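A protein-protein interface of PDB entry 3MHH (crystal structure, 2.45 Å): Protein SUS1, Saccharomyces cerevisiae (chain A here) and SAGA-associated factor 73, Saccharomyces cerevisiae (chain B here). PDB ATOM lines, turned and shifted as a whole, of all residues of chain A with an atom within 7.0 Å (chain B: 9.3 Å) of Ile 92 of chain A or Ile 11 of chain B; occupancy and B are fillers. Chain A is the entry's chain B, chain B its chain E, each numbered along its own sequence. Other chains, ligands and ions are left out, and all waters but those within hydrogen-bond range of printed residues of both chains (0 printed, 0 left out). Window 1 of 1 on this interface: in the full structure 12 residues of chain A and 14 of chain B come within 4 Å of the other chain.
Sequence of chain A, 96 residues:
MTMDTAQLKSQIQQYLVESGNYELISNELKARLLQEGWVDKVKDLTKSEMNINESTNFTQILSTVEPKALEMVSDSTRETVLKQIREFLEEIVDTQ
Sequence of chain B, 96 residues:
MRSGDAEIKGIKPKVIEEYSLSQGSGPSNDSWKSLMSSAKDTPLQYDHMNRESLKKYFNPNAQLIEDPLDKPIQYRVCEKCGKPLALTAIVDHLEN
Ile 92 of chain A touches three residues of chain B.
Ile 11 of chain B touches just one residue of chain A: Ile 92 (3.3 Å).
Of chain B, only Gly 10 (3.6 Å) and Lys 12 (3.0 Å) come within 4 Å of Val 93 of chain A.
Printed residues of chain A within 4 Å of Leu 21 of chain B: Gln 11 (3.3 Å).
Printed residues of chain A within 4 Å of Ser 22 of chain B: Gln 11 (3.99 Å).
Of the printed residues of chain A, Gly 10 of chain B touches Val 93 and Asp 94.
Glu 87 of chain A touches none of the printed residues of chain B.
The nearest residue of chain A that does not touch Ile 11 of chain B is Gln 11 of chain A (4.1 Å).
The side-chain carboxylate (OD1) of Asp 94 of chain A is in salt-bridge range of the side-chain amino group (NZ) of Lys 12 of chain B, at 2.7 Å.
The backbone carbonyl oxygen of Val 93 of chain A is in hydrogen-bond range of the side-chain amino group of Lys 12 of chain B, 3.0 Å away.
The side-chain amide oxygen of Gln 11 of chain A lies close to the backbone carbonyl oxygen of Leu 21 of chain B (3.3 Å).
N of Asp 94 of chain A sits at hydrogen-bond distance from O of Gly 10 of chain B (2.9 Å).
OE1 of Gln 11 of chain A is in hydrogen-bond range of NE2 of Gln 23 of chain B (2.7 Å).
The backbone NH (N) of Lys 12 of chain B sits at hydrogen-bond distance from the backbone carbonyl oxygen (O) of Ile 92 of chain A (2.8 Å).
The side-chain carboxylate (OD2) of Asp 94 of chain A lies within salt-bridge range of the side-chain amino group (NZ) of Lys 9 of chain B (2.9 Å).
Hydrophobic or aromatic side chains of chain B that line the printed part of chain A: Ile 8, Ile 11, Pro 13, Val 15, Tyr 19 and Leu 21.
Of the 14 printed residues of chain A, 6 touch a printed residue of chain B.
Hydrophobic or aromatic side chains of chain A that line the printed part of chain B: Tyr 15, Ile 92 and Val 93.
Among the printed residues, 15 pairs touch across the chains.
Among the printed residues, Asp or Glu carboxylates within 4 Å of a Lys or Arg side-chain nitrogen of the other chain: Asp 94 of chain A with Lys 9 of chain B and Asp 94 of chain A with Lys 12 of chain B.
The backbone carbonyl oxygen of Ile 16 of chain B lies within hydrogen-bond range of the backbone NH of Leu 21 of chain B.
Among the printed residues, pairs that only touch across the chains: Ile 92 of chain A with Ile 11 of chain B, Val 93 of chain A with Gly 10 of chain B, Asp 94 of chain A with Ile 8 of chain B, Glu 91 of chain A with Lys 12 of chain B, Tyr 15 of chain A with Tyr 19 of chain B, Asp 94 of chain A with Pro 13 of chain B, Ile 92 of chain A with Val 15 of chain B and Gln 11 of chain A with Ser 22 of chain B.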
ATOM      1  N   LEU A   8     -26.634  18.245   6.348  1.00  0.00           N
ATOM      2  CA  LEU A   8     -27.171  17.029   5.774  1.00  0.00           C
ATOM      3  C   LEU A   8     -26.044  16.077   5.403  1.00  0.00           C
ATOM      4  O   LEU A   8     -26.120  14.867   5.651  1.00  0.00           O
ATOM      5  CB  LEU A   8     -27.982  17.382   4.528  1.00  0.00           C
ATOM      6  CG  LEU A   8     -28.747  16.261   3.834  1.00  0.00           C
ATOM      7  CD1 LEU A   8     -29.708  15.586   4.806  1.00  0.00           C
ATOM      8  CD2 LEU A   8     -29.501  16.839   2.643  1.00  0.00           C
ATOM      9  N   GLN A  11     -24.091  14.643   8.452  1.00  0.00           N
ATOM     10  CA  GLN A  11     -24.971  13.733   9.177  1.00  0.00           C
ATOM     11  C   GLN A  11     -25.047  12.376   8.507  1.00  0.00           C
ATOM     12  O   GLN A  11     -25.056  11.344   9.176  1.00  0.00           O
ATOM     13  CB  GLN A  11     -26.376  14.319   9.299  1.00  0.00           C
ATOM     14  CG  GLN A  11     -26.526  15.323  10.424  1.00  0.00           C
ATOM     15  CD  GLN A  11     -27.958  15.814  10.598  1.00  0.00           C
ATOM     16  OE1 GLN A  11     -28.401  16.080  11.718  1.00  0.00           O
ATOM     17  NE2 GLN A  11     -28.692  15.920   9.492  1.00  0.00           N
ATOM     18  N   ILE A  12     -25.129  12.389   7.183  1.00  0.00           N
ATOM     19  CA  ILE A  12     -25.158  11.169   6.398  1.00  0.00           C
ATOM     20  C   ILE A  12     -23.840  10.410   6.508  1.00  0.00           C
ATOM     21  O   ILE A  12     -23.825   9.175   6.637  1.00  0.00           O
ATOM     22  CB  ILE A  12     -25.445  11.482   4.920  1.00  0.00           C
ATOM     23  CG1 ILE A  12     -26.915  11.873   4.756  1.00  0.00           C
ATOM     24  CG2 ILE A  12     -25.117  10.278   4.037  1.00  0.00           C
ATOM     25  CD1 ILE A  12     -27.295  12.217   3.342  1.00  0.00           C
ATOM     26  N   GLN A  13     -22.733  11.141   6.479  1.00  0.00           N
ATOM     27  CA  GLN A  13     -21.419  10.513   6.606  1.00  0.00           C
ATOM     28  C   GLN A  13     -21.259   9.874   7.963  1.00  0.00           C
ATOM     29  O   GLN A  13     -20.638   8.823   8.098  1.00  0.00           O
ATOM     30  CB  GLN A  13     -20.317  11.534   6.411  1.00  0.00           C
ATOM     31  CG  GLN A  13     -20.161  11.988   4.986  1.00  0.00           C
ATOM     32  CD  GLN A  13     -19.105  13.046   4.855  1.00  0.00           C
ATOM     33  OE1 GLN A  13     -18.171  12.918   4.049  1.00  0.00           O
ATOM     34  NE2 GLN A  13     -19.214  14.086   5.669  1.00  0.00           N
ATOM     35  N   TYR A  15     -23.656   8.580   9.649  1.00  0.00           N
ATOM     36  CA  TYR A  15     -24.390   7.325   9.581  1.00  0.00           C
ATOM     37  C   TYR A  15     -23.562   6.268   8.858  1.00  0.00           C
ATOM     38  O   TYR A  15     -23.481   5.123   9.298  1.00  0.00           O
ATOM     39  CB  TYR A  15     -25.729   7.497   8.859  1.00  0.00           C
ATOM     40  CG  TYR A  15     -26.215   6.212   8.243  1.00  0.00           C
ATOM     41  CD1 TYR A  15     -26.815   5.232   9.024  1.00  0.00           C
ATOM     42  CD2 TYR A  15     -26.026   5.951   6.893  1.00  0.00           C
ATOM     43  CE1 TYR A  15     -27.228   4.044   8.483  1.00  0.00           C
ATOM     44  CE2 TYR A  15     -26.451   4.761   6.331  1.00  0.00           C
ATOM     45  CZ  TYR A  15     -27.046   3.812   7.132  1.00  0.00           C
ATOM     46  OH  TYR A  15     -27.459   2.626   6.588  1.00  0.00           O
ATOM     47  N   LEU A  16     -22.953   6.654   7.744  1.00  0.00           N
ATOM     48  CA  LEU A  16     -22.213   5.695   6.932  1.00  0.00           C
ATOM     49  C   LEU A  16     -21.092   5.099   7.758  1.00  0.00           C
ATOM     50  O   LEU A  16     -20.913   3.875   7.782  1.00  0.00           O
ATOM     51  CB  LEU A  16     -21.663   6.341   5.653  1.00  0.00           C
ATOM     52  CG  LEU A  16     -22.697   6.687   4.570  1.00  0.00           C
ATOM     53  CD1 LEU A  16     -22.049   7.381   3.357  1.00  0.00           C
ATOM     54  CD2 LEU A  16     -23.457   5.460   4.122  1.00  0.00           C
ATOM     55  N   GLU A  87     -27.092   3.628  -3.267  1.00  0.00           N
ATOM     56  CA  GLU A  87     -27.948   2.596  -2.725  1.00  0.00           C
ATOM     57  C   GLU A  87     -27.966   2.707  -1.207  1.00  0.00           C
ATOM     58  O   GLU A  87     -29.011   2.606  -0.579  1.00  0.00           O
ATOM     59  CB  GLU A  87     -27.484   1.216  -3.179  1.00  0.00           C
ATOM     60  CG  GLU A  87     -27.826   0.867  -4.638  1.00  0.00           C
ATOM     61  CD  GLU A  87     -27.124  -0.404  -5.135  1.00  0.00           C
ATOM     62  OE1 GLU A  87     -27.667  -1.051  -6.038  1.00  0.00           O
ATOM     63  OE2 GLU A  87     -26.021  -0.755  -4.637  1.00  0.00           O
ATOM     64  N   PHE A  88     -26.813   2.969  -0.611  1.00  0.00           N
ATOM     65  CA  PHE A  88     -26.764   3.138   0.829  1.00  0.00           C
ATOM     66  C   PHE A  88     -27.649   4.294   1.281  1.00  0.00           C
ATOM     67  O   PHE A  88     -28.393   4.154   2.248  1.00  0.00           O
ATOM     68  CB  PHE A  88     -25.329   3.314   1.302  1.00  0.00           C
ATOM     69  CG  PHE A  88     -24.559   2.020   1.408  1.00  0.00           C
ATOM     70  CD1 PHE A  88     -25.046   0.970   2.175  1.00  0.00           C
ATOM     71  CD2 PHE A  88     -23.330   1.871   0.780  1.00  0.00           C
ATOM     72  CE1 PHE A  88     -24.330  -0.218   2.293  1.00  0.00           C
ATOM     73  CE2 PHE A  88     -22.599   0.693   0.896  1.00  0.00           C
ATOM     74  CZ  PHE A  88     -23.100  -0.355   1.650  1.00  0.00           C
ATOM     75  N   LEU A  89     -27.624   5.407   0.551  1.00  0.00           N
ATOM     76  CA  LEU A  89     -28.453   6.574   0.894  1.00  0.00           C
ATOM     77  C   LEU A  89     -29.934   6.344   0.602  1.00  0.00           C
ATOM     78  O   LEU A  89     -30.793   6.858   1.307  1.00  0.00           O
ATOM     79  CB  LEU A  89     -27.982   7.820   0.137  1.00  0.00           C
ATOM     80  CG  LEU A  89     -26.603   8.368   0.511  1.00  0.00           C
ATOM     81  CD1 LEU A  89     -26.240   9.558  -0.347  1.00  0.00           C
ATOM     82  CD2 LEU A  89     -26.593   8.756   1.971  1.00  0.00           C
ATOM     83  N   GLU A  90     -30.233   5.589  -0.448  1.00  0.00           N
ATOM     84  CA  GLU A  90     -31.622   5.259  -0.772  1.00  0.00           C
ATOM     85  C   GLU A  90     -32.335   4.726   0.469  1.00  0.00           C
ATOM     86  O   GLU A  90     -33.534   4.886   0.634  1.00  0.00           O
ATOM     87  CB  GLU A  90     -31.670   4.204  -1.883  1.00  0.00           C
ATOM     88  CG  GLU A  90     -31.672   4.770  -3.310  1.00  0.00           C
ATOM     89  CD  GLU A  90     -31.388   3.711  -4.377  1.00  0.00           C
ATOM     90  OE1 GLU A  90     -30.884   4.083  -5.457  1.00  0.00           O
ATOM     91  OE2 GLU A  90     -31.658   2.513  -4.136  1.00  0.00           O
ATOM     92  N   GLU A  91     -31.557   4.118   1.346  1.00  0.00           N
ATOM     93  CA  GLU A  91     -32.049   3.405   2.503  1.00  0.00           C
ATOM     94  C   GLU A  91     -32.425   4.352   3.643  1.00  0.00           C
ATOM     95  O   GLU A  91     -33.245   4.000   4.490  1.00  0.00           O
ATOM     96  CB  GLU A  91     -30.925   2.466   2.975  1.00  0.00           C
ATOM     97  CG  GLU A  91     -31.345   1.085   3.419  1.00  0.00           C
ATOM     98  CD  GLU A  91     -30.218   0.068   3.288  1.00  0.00           C
ATOM     99  OE1 GLU A  91     -29.115   0.306   3.825  1.00  0.00           O
ATOM    100  OE2 GLU A  91     -30.437  -0.973   2.642  1.00  0.00           O
ATOM    101  N   ILE A  92     -31.816   5.537   3.680  1.00  0.00           N
ATOM    102  CA  ILE A  92     -31.956   6.430   4.834  1.00  0.00           C
ATOM    103  C   ILE A  92     -32.409   7.857   4.525  1.00  0.00           C
ATOM    104  O   ILE A  92     -32.548   8.663   5.444  1.00  0.00           O
ATOM    105  CB  ILE A  92     -30.631   6.543   5.628  1.00  0.00           C
ATOM    106  CG1 ILE A  92     -29.623   7.399   4.853  1.00  0.00           C
ATOM    107  CG2 ILE A  92     -30.065   5.147   5.950  1.00  0.00           C
ATOM    108  CD1 ILE A  92     -28.412   7.768   5.645  1.00  0.00           C
ATOM    109  N   VAL A  93     -32.619   8.206   3.258  1.00  0.00           N
ATOM    110  CA  VAL A  93     -33.160   9.535   2.961  1.00  0.00           C
ATOM    111  C   VAL A  93     -34.581   9.430   2.442  1.00  0.00           C
ATOM    112  O   VAL A  93     -34.975   8.402   1.893  1.00  0.00           O
ATOM    113  CB  VAL A  93     -32.299  10.327   1.941  1.00  0.00           C
ATOM    114  CG1 VAL A  93     -30.833  10.207   2.279  1.00  0.00           C
ATOM    115  CG2 VAL A  93     -32.582   9.875   0.512  1.00  0.00           C
ATOM    116  N   ASP A  94     -35.359  10.487   2.645  1.00  0.00           N
ATOM    117  CA  ASP A  94     -36.684  10.576   2.049  1.00  0.00           C
ATOM    118  C   ASP A  94     -36.621  11.592   0.929  1.00  0.00           C
ATOM    119  O   ASP A  94     -35.821  12.526   0.977  1.00  0.00           O
ATOM    120  CB  ASP A  94     -37.718  11.008   3.083  1.00  0.00           C
ATOM    121  CG  ASP A  94     -37.916   9.979   4.164  1.00  0.00           C
ATOM    122  OD1 ASP A  94     -37.936   8.775   3.831  1.00  0.00           O
ATOM    123  OD2 ASP A  94     -38.049  10.368   5.346  1.00  0.00           O
ATOM    124  N   ILE B   8     -34.040  15.794  -2.062  1.00  0.00           N
ATOM    125  CA  ILE B   8     -34.056  15.196  -0.728  1.00  0.00           C
ATOM    126  C   ILE B   8     -34.869  16.024   0.269  1.00  0.00           C
ATOM    127  O   ILE B   8     -34.634  17.217   0.419  1.00  0.00           O
ATOM    128  CB  ILE B   8     -32.633  15.032  -0.178  1.00  0.00           C
ATOM    129  CG1 ILE B   8     -31.866  14.005  -1.009  1.00  0.00           C
ATOM    130  CG2 ILE B   8     -32.679  14.586   1.275  1.00  0.00           C
ATOM    131  CD1 ILE B   8     -30.389  13.943  -0.696  1.00  0.00           C
ATOM    132  N   LYS B   9     -35.828  15.393   0.940  1.00  0.00           N
ATOM    133  CA  LYS B   9     -36.574  16.054   2.009  1.00  0.00           C
ATOM    134  C   LYS B   9     -35.700  16.178   3.248  1.00  0.00           C
ATOM    135  O   LYS B   9     -35.577  17.242   3.846  1.00  0.00           O
ATOM    136  CB  LYS B   9     -37.837  15.268   2.372  1.00  0.00           C
ATOM    137  CG  LYS B   9     -38.442  15.691   3.715  1.00  0.00           C
ATOM    138  CD  LYS B   9     -39.737  14.943   4.064  1.00  0.00           C
ATOM    139  CE  LYS B   9     -39.490  13.473   4.432  1.00  0.00           C
ATOM    140  NZ  LYS B   9     -38.406  13.247   5.450  1.00  0.00           N
ATOM    141  N   GLY B  10     -35.107  15.063   3.633  1.00  0.00           N
ATOM    142  CA  GLY B  10     -34.287  15.000   4.826  1.00  0.00           C
ATOM    143  C   GLY B  10     -33.905  13.558   5.035  1.00  0.00           C
ATOM    144  O   GLY B  10     -34.254  12.693   4.230  1.00  0.00           O
ATOM    145  N   ILE B  11     -33.171  13.293   6.102  1.00  0.00           N
ATOM    146  CA  ILE B  11     -32.868  11.926   6.450  1.00  0.00           C
ATOM    147  C   ILE B  11     -33.999  11.364   7.298  1.00  0.00           C
ATOM    148  O   ILE B  11     -34.602  12.075   8.111  1.00  0.00           O
ATOM    149  CB  ILE B  11     -31.500  11.796   7.158  1.00  0.00           C
ATOM    150  CG1 ILE B  11     -31.453  10.512   7.985  1.00  0.00           C
ATOM    151  CG2 ILE B  11     -31.219  13.017   8.027  1.00  0.00           C
ATOM    152  CD1 ILE B  11     -30.097  10.219   8.541  1.00  0.00           C
ATOM    153  N   LYS B  12     -34.315  10.092   7.073  1.00  0.00           N
ATOM    154  CA  LYS B  12     -35.379   9.445   7.819  1.00  0.00           C
ATOM    155  C   LYS B  12     -35.246   9.761   9.300  1.00  0.00           C
ATOM    156  O   LYS B  12     -34.186   9.552   9.899  1.00  0.00           O
ATOM    157  CB  LYS B  12     -35.374   7.932   7.595  1.00  0.00           C
ATOM    158  CG  LYS B  12     -35.893   7.522   6.229  1.00  0.00           C
ATOM    159  CD  LYS B  12     -35.857   6.022   6.027  1.00  0.00           C
ATOM    160  CE  LYS B  12     -36.716   5.612   4.838  1.00  0.00           C
ATOM    161  NZ  LYS B  12     -36.477   6.478   3.652  1.00  0.00           N
ATOM    162  N   PRO B  13     -36.324  10.288   9.890  1.00  0.00           N
ATOM    163  CA  PRO B  13     -36.373  10.527  11.317  1.00  0.00           C
ATOM    164  C   PRO B  13     -35.922   9.301  12.094  1.00  0.00           C
ATOM    165  O   PRO B  13     -35.148   9.420  13.036  1.00  0.00           O
ATOM    166  CB  PRO B  13     -37.853  10.810  11.574  1.00  0.00           C
ATOM    167  CG  PRO B  13     -38.369  11.349  10.276  1.00  0.00           C
ATOM    168  CD  PRO B  13     -37.593  10.639   9.219  1.00  0.00           C
ATOM    169  N   LYS B  14     -36.393   8.129  11.689  1.00  0.00           N
ATOM    170  CA  LYS B  14     -36.079   6.896  12.409  1.00  0.00           C
ATOM    171  C   LYS B  14     -34.572   6.712  12.445  1.00  0.00           C
ATOM    172  O   LYS B  14     -34.016   6.318  13.462  1.00  0.00           O
ATOM    173  CB  LYS B  14     -36.772   5.695  11.753  1.00  0.00           C
ATOM    174  CG  LYS B  14     -36.383   4.323  12.307  1.00  0.00           C
ATOM    175  CD  LYS B  14     -36.834   4.112  13.743  1.00  0.00           C
ATOM    176  CE  LYS B  14     -36.477   2.710  14.246  1.00  0.00           C
ATOM    177  NZ  LYS B  14     -35.064   2.332  13.912  1.00  0.00           N
ATOM    178  N   VAL B  15     -33.912   7.026  11.335  1.00  0.00           N
ATOM    179  CA  VAL B  15     -32.464   6.896  11.238  1.00  0.00           C
ATOM    180  C   VAL B  15     -31.767   7.971  12.066  1.00  0.00           C
ATOM    181  O   VAL B  15     -30.760   7.705  12.722  1.00  0.00           O
ATOM    182  CB  VAL B  15     -31.989   7.005   9.783  1.00  0.00           C
ATOM    183  CG1 VAL B  15     -30.463   6.951   9.718  1.00  0.00           C
ATOM    184  CG2 VAL B  15     -32.605   5.895   8.942  1.00  0.00           C
ATOM    185  N   ILE B  16     -32.306   9.187  12.042  1.00  0.00           N
ATOM    186  CA  ILE B  16     -31.764  10.260  12.870  1.00  0.00           C
ATOM    187  C   ILE B  16     -31.666   9.803  14.317  1.00  0.00           C
ATOM    188  O   ILE B  16     -30.655  10.045  14.976  1.00  0.00           O
ATOM    189  CB  ILE B  16     -32.624  11.536  12.802  1.00  0.00           C
ATOM    190  CG1 ILE B  16     -32.264  12.359  11.564  1.00  0.00           C
ATOM    191  CG2 ILE B  16     -32.413  12.394  14.038  1.00  0.00           C
ATOM    192  CD1 ILE B  16     -33.028  13.650  11.459  1.00  0.00           C
ATOM    193  N   GLU B  17     -32.709   9.121  14.792  1.00  0.00           N
ATOM    194  CA  GLU B  17     -32.803   8.703  16.191  1.00  0.00           C
ATOM    195  C   GLU B  17     -31.861   7.547  16.520  1.00  0.00           C
ATOM    196  O   GLU B  17     -31.154   7.590  17.523  1.00  0.00           O
ATOM    197  CB  GLU B  17     -34.247   8.315  16.536  1.00  0.00           C
ATOM    198  CG  GLU B  17     -34.458   7.932  18.004  1.00  0.00           C
ATOM    199  CD  GLU B  17     -35.923   7.978  18.425  1.00  0.00           C
ATOM    200  OE1 GLU B  17     -36.692   7.059  18.055  1.00  0.00           O
ATOM    201  OE2 GLU B  17     -36.302   8.931  19.142  1.00  0.00           O
ATOM    202  N   GLU B  18     -31.872   6.516  15.680  1.00  0.00           N
ATOM    203  CA  GLU B  18     -31.010   5.354  15.855  1.00  0.00           C
ATOM    204  C   GLU B  18     -29.560   5.751  16.061  1.00  0.00           C
ATOM    205  O   GLU B  18     -28.884   5.245  16.954  1.00  0.00           O
ATOM    206  CB  GLU B  18     -31.069   4.464  14.618  1.00  0.00           C
ATOM    207  CG  GLU B  18     -32.143   3.399  14.622  1.00  0.00           C
ATOM    208  CD  GLU B  18     -32.066   2.527  13.373  1.00  0.00           C
ATOM    209  OE1 GLU B  18     -32.596   2.956  12.319  1.00  0.00           O
ATOM    210  OE2 GLU B  18     -31.463   1.425  13.445  1.00  0.00           O
ATOM    211  N   TYR B  19     -29.082   6.652  15.212  1.00  0.00           N
ATOM    212  CA  TYR B  19     -27.671   6.988  15.173  1.00  0.00           C
ATOM    213  C   TYR B  19     -27.359   8.306  15.865  1.00  0.00           C
ATOM    214  O   TYR B  19     -26.245   8.812  15.770  1.00  0.00           O
ATOM    215  CB  TYR B  19     -27.207   7.006  13.727  1.00  0.00           C
ATOM    216  CG  TYR B  19     -27.210   5.627  13.129  1.00  0.00           C
ATOM    217  CD1 TYR B  19     -26.059   4.840  13.137  1.00  0.00           C
ATOM    218  CD2 TYR B  19     -28.367   5.085  12.599  1.00  0.00           C
ATOM    219  CE1 TYR B  19     -26.062   3.569  12.623  1.00  0.00           C
ATOM    220  CE2 TYR B  19     -28.375   3.801  12.084  1.00  0.00           C
ATOM    221  CZ  TYR B  19     -27.222   3.052  12.101  1.00  0.00           C
ATOM    222  OH  TYR B  19     -27.226   1.785  11.581  1.00  0.00           O
ATOM    223  N   SER B  20     -28.338   8.847  16.585  1.00  0.00           N
ATOM    224  CA  SER B  20     -28.150  10.095  17.326  1.00  0.00           C
ATOM    225  C   SER B  20     -27.456  11.110  16.422  1.00  0.00           C
ATOM    226  O   SER B  20     -26.381  11.614  16.739  1.00  0.00           O
ATOM    227  CB  SER B  20     -27.325   9.851  18.592  1.00  0.00           C
ATOM    228  OG  SER B  20     -27.753   8.680  19.270  1.00  0.00           O
ATOM    229  N   LEU B  21     -28.086  11.397  15.291  1.00  0.00           N
ATOM    230  CA  LEU B  21     -27.502  12.279  14.290  1.00  0.00           C
ATOM    231  C   LEU B  21     -27.653  13.772  14.606  1.00  0.00           C
ATOM    232  O   LEU B  21     -26.801  14.569  14.237  1.00  0.00           O
ATOM    233  CB  LEU B  21     -28.103  11.975  12.921  1.00  0.00           C
ATOM    234  CG  LEU B  21     -27.259  11.116  11.990  1.00  0.00           C
ATOM    235  CD1 LEU B  21     -26.443  10.068  12.741  1.00  0.00           C
ATOM    236  CD2 LEU B  21     -28.155  10.476  10.945  1.00  0.00           C
ATOM    237  N   SER B  22     -28.745  14.152  15.259  1.00  0.00           N
ATOM    238  CA  SER B  22     -28.956  15.548  15.638  1.00  0.00           C
ATOM    239  C   SER B  22     -27.756  16.081  16.422  1.00  0.00           C
ATOM    240  O   SER B  22     -27.429  15.569  17.496  1.00  0.00           O
ATOM    241  CB  SER B  22     -30.237  15.675  16.463  1.00  0.00           C
ATOM    242  OG  SER B  22     -30.586  14.424  17.037  1.00  0.00           O
ATOM    243  N   GLN B  23     -27.101  17.107  15.883  1.00  0.00           N
ATOM    244  CA  GLN B  23     -25.869  17.627  16.479  1.00  0.00           C
ATOM    245  C   GLN B  23     -25.880  19.143  16.686  1.00  0.00           C
ATOM    246  O   GLN B  23     -26.886  19.814  16.442  1.00  0.00           O
ATOM    247  CB  GLN B  23     -24.647  17.223  15.639  1.00  0.00           C
ATOM    248  CG  GLN B  23     -24.946  16.822  14.188  1.00  0.00           C
ATOM    249  CD  GLN B  23     -25.400  17.978  13.311  1.00  0.00           C
ATOM    250  OE1 GLN B  23     -24.726  19.008  13.209  1.00  0.00           O
ATOM    251  NE2 GLN B  23     -26.539  17.798  12.648  1.00  0.00           N
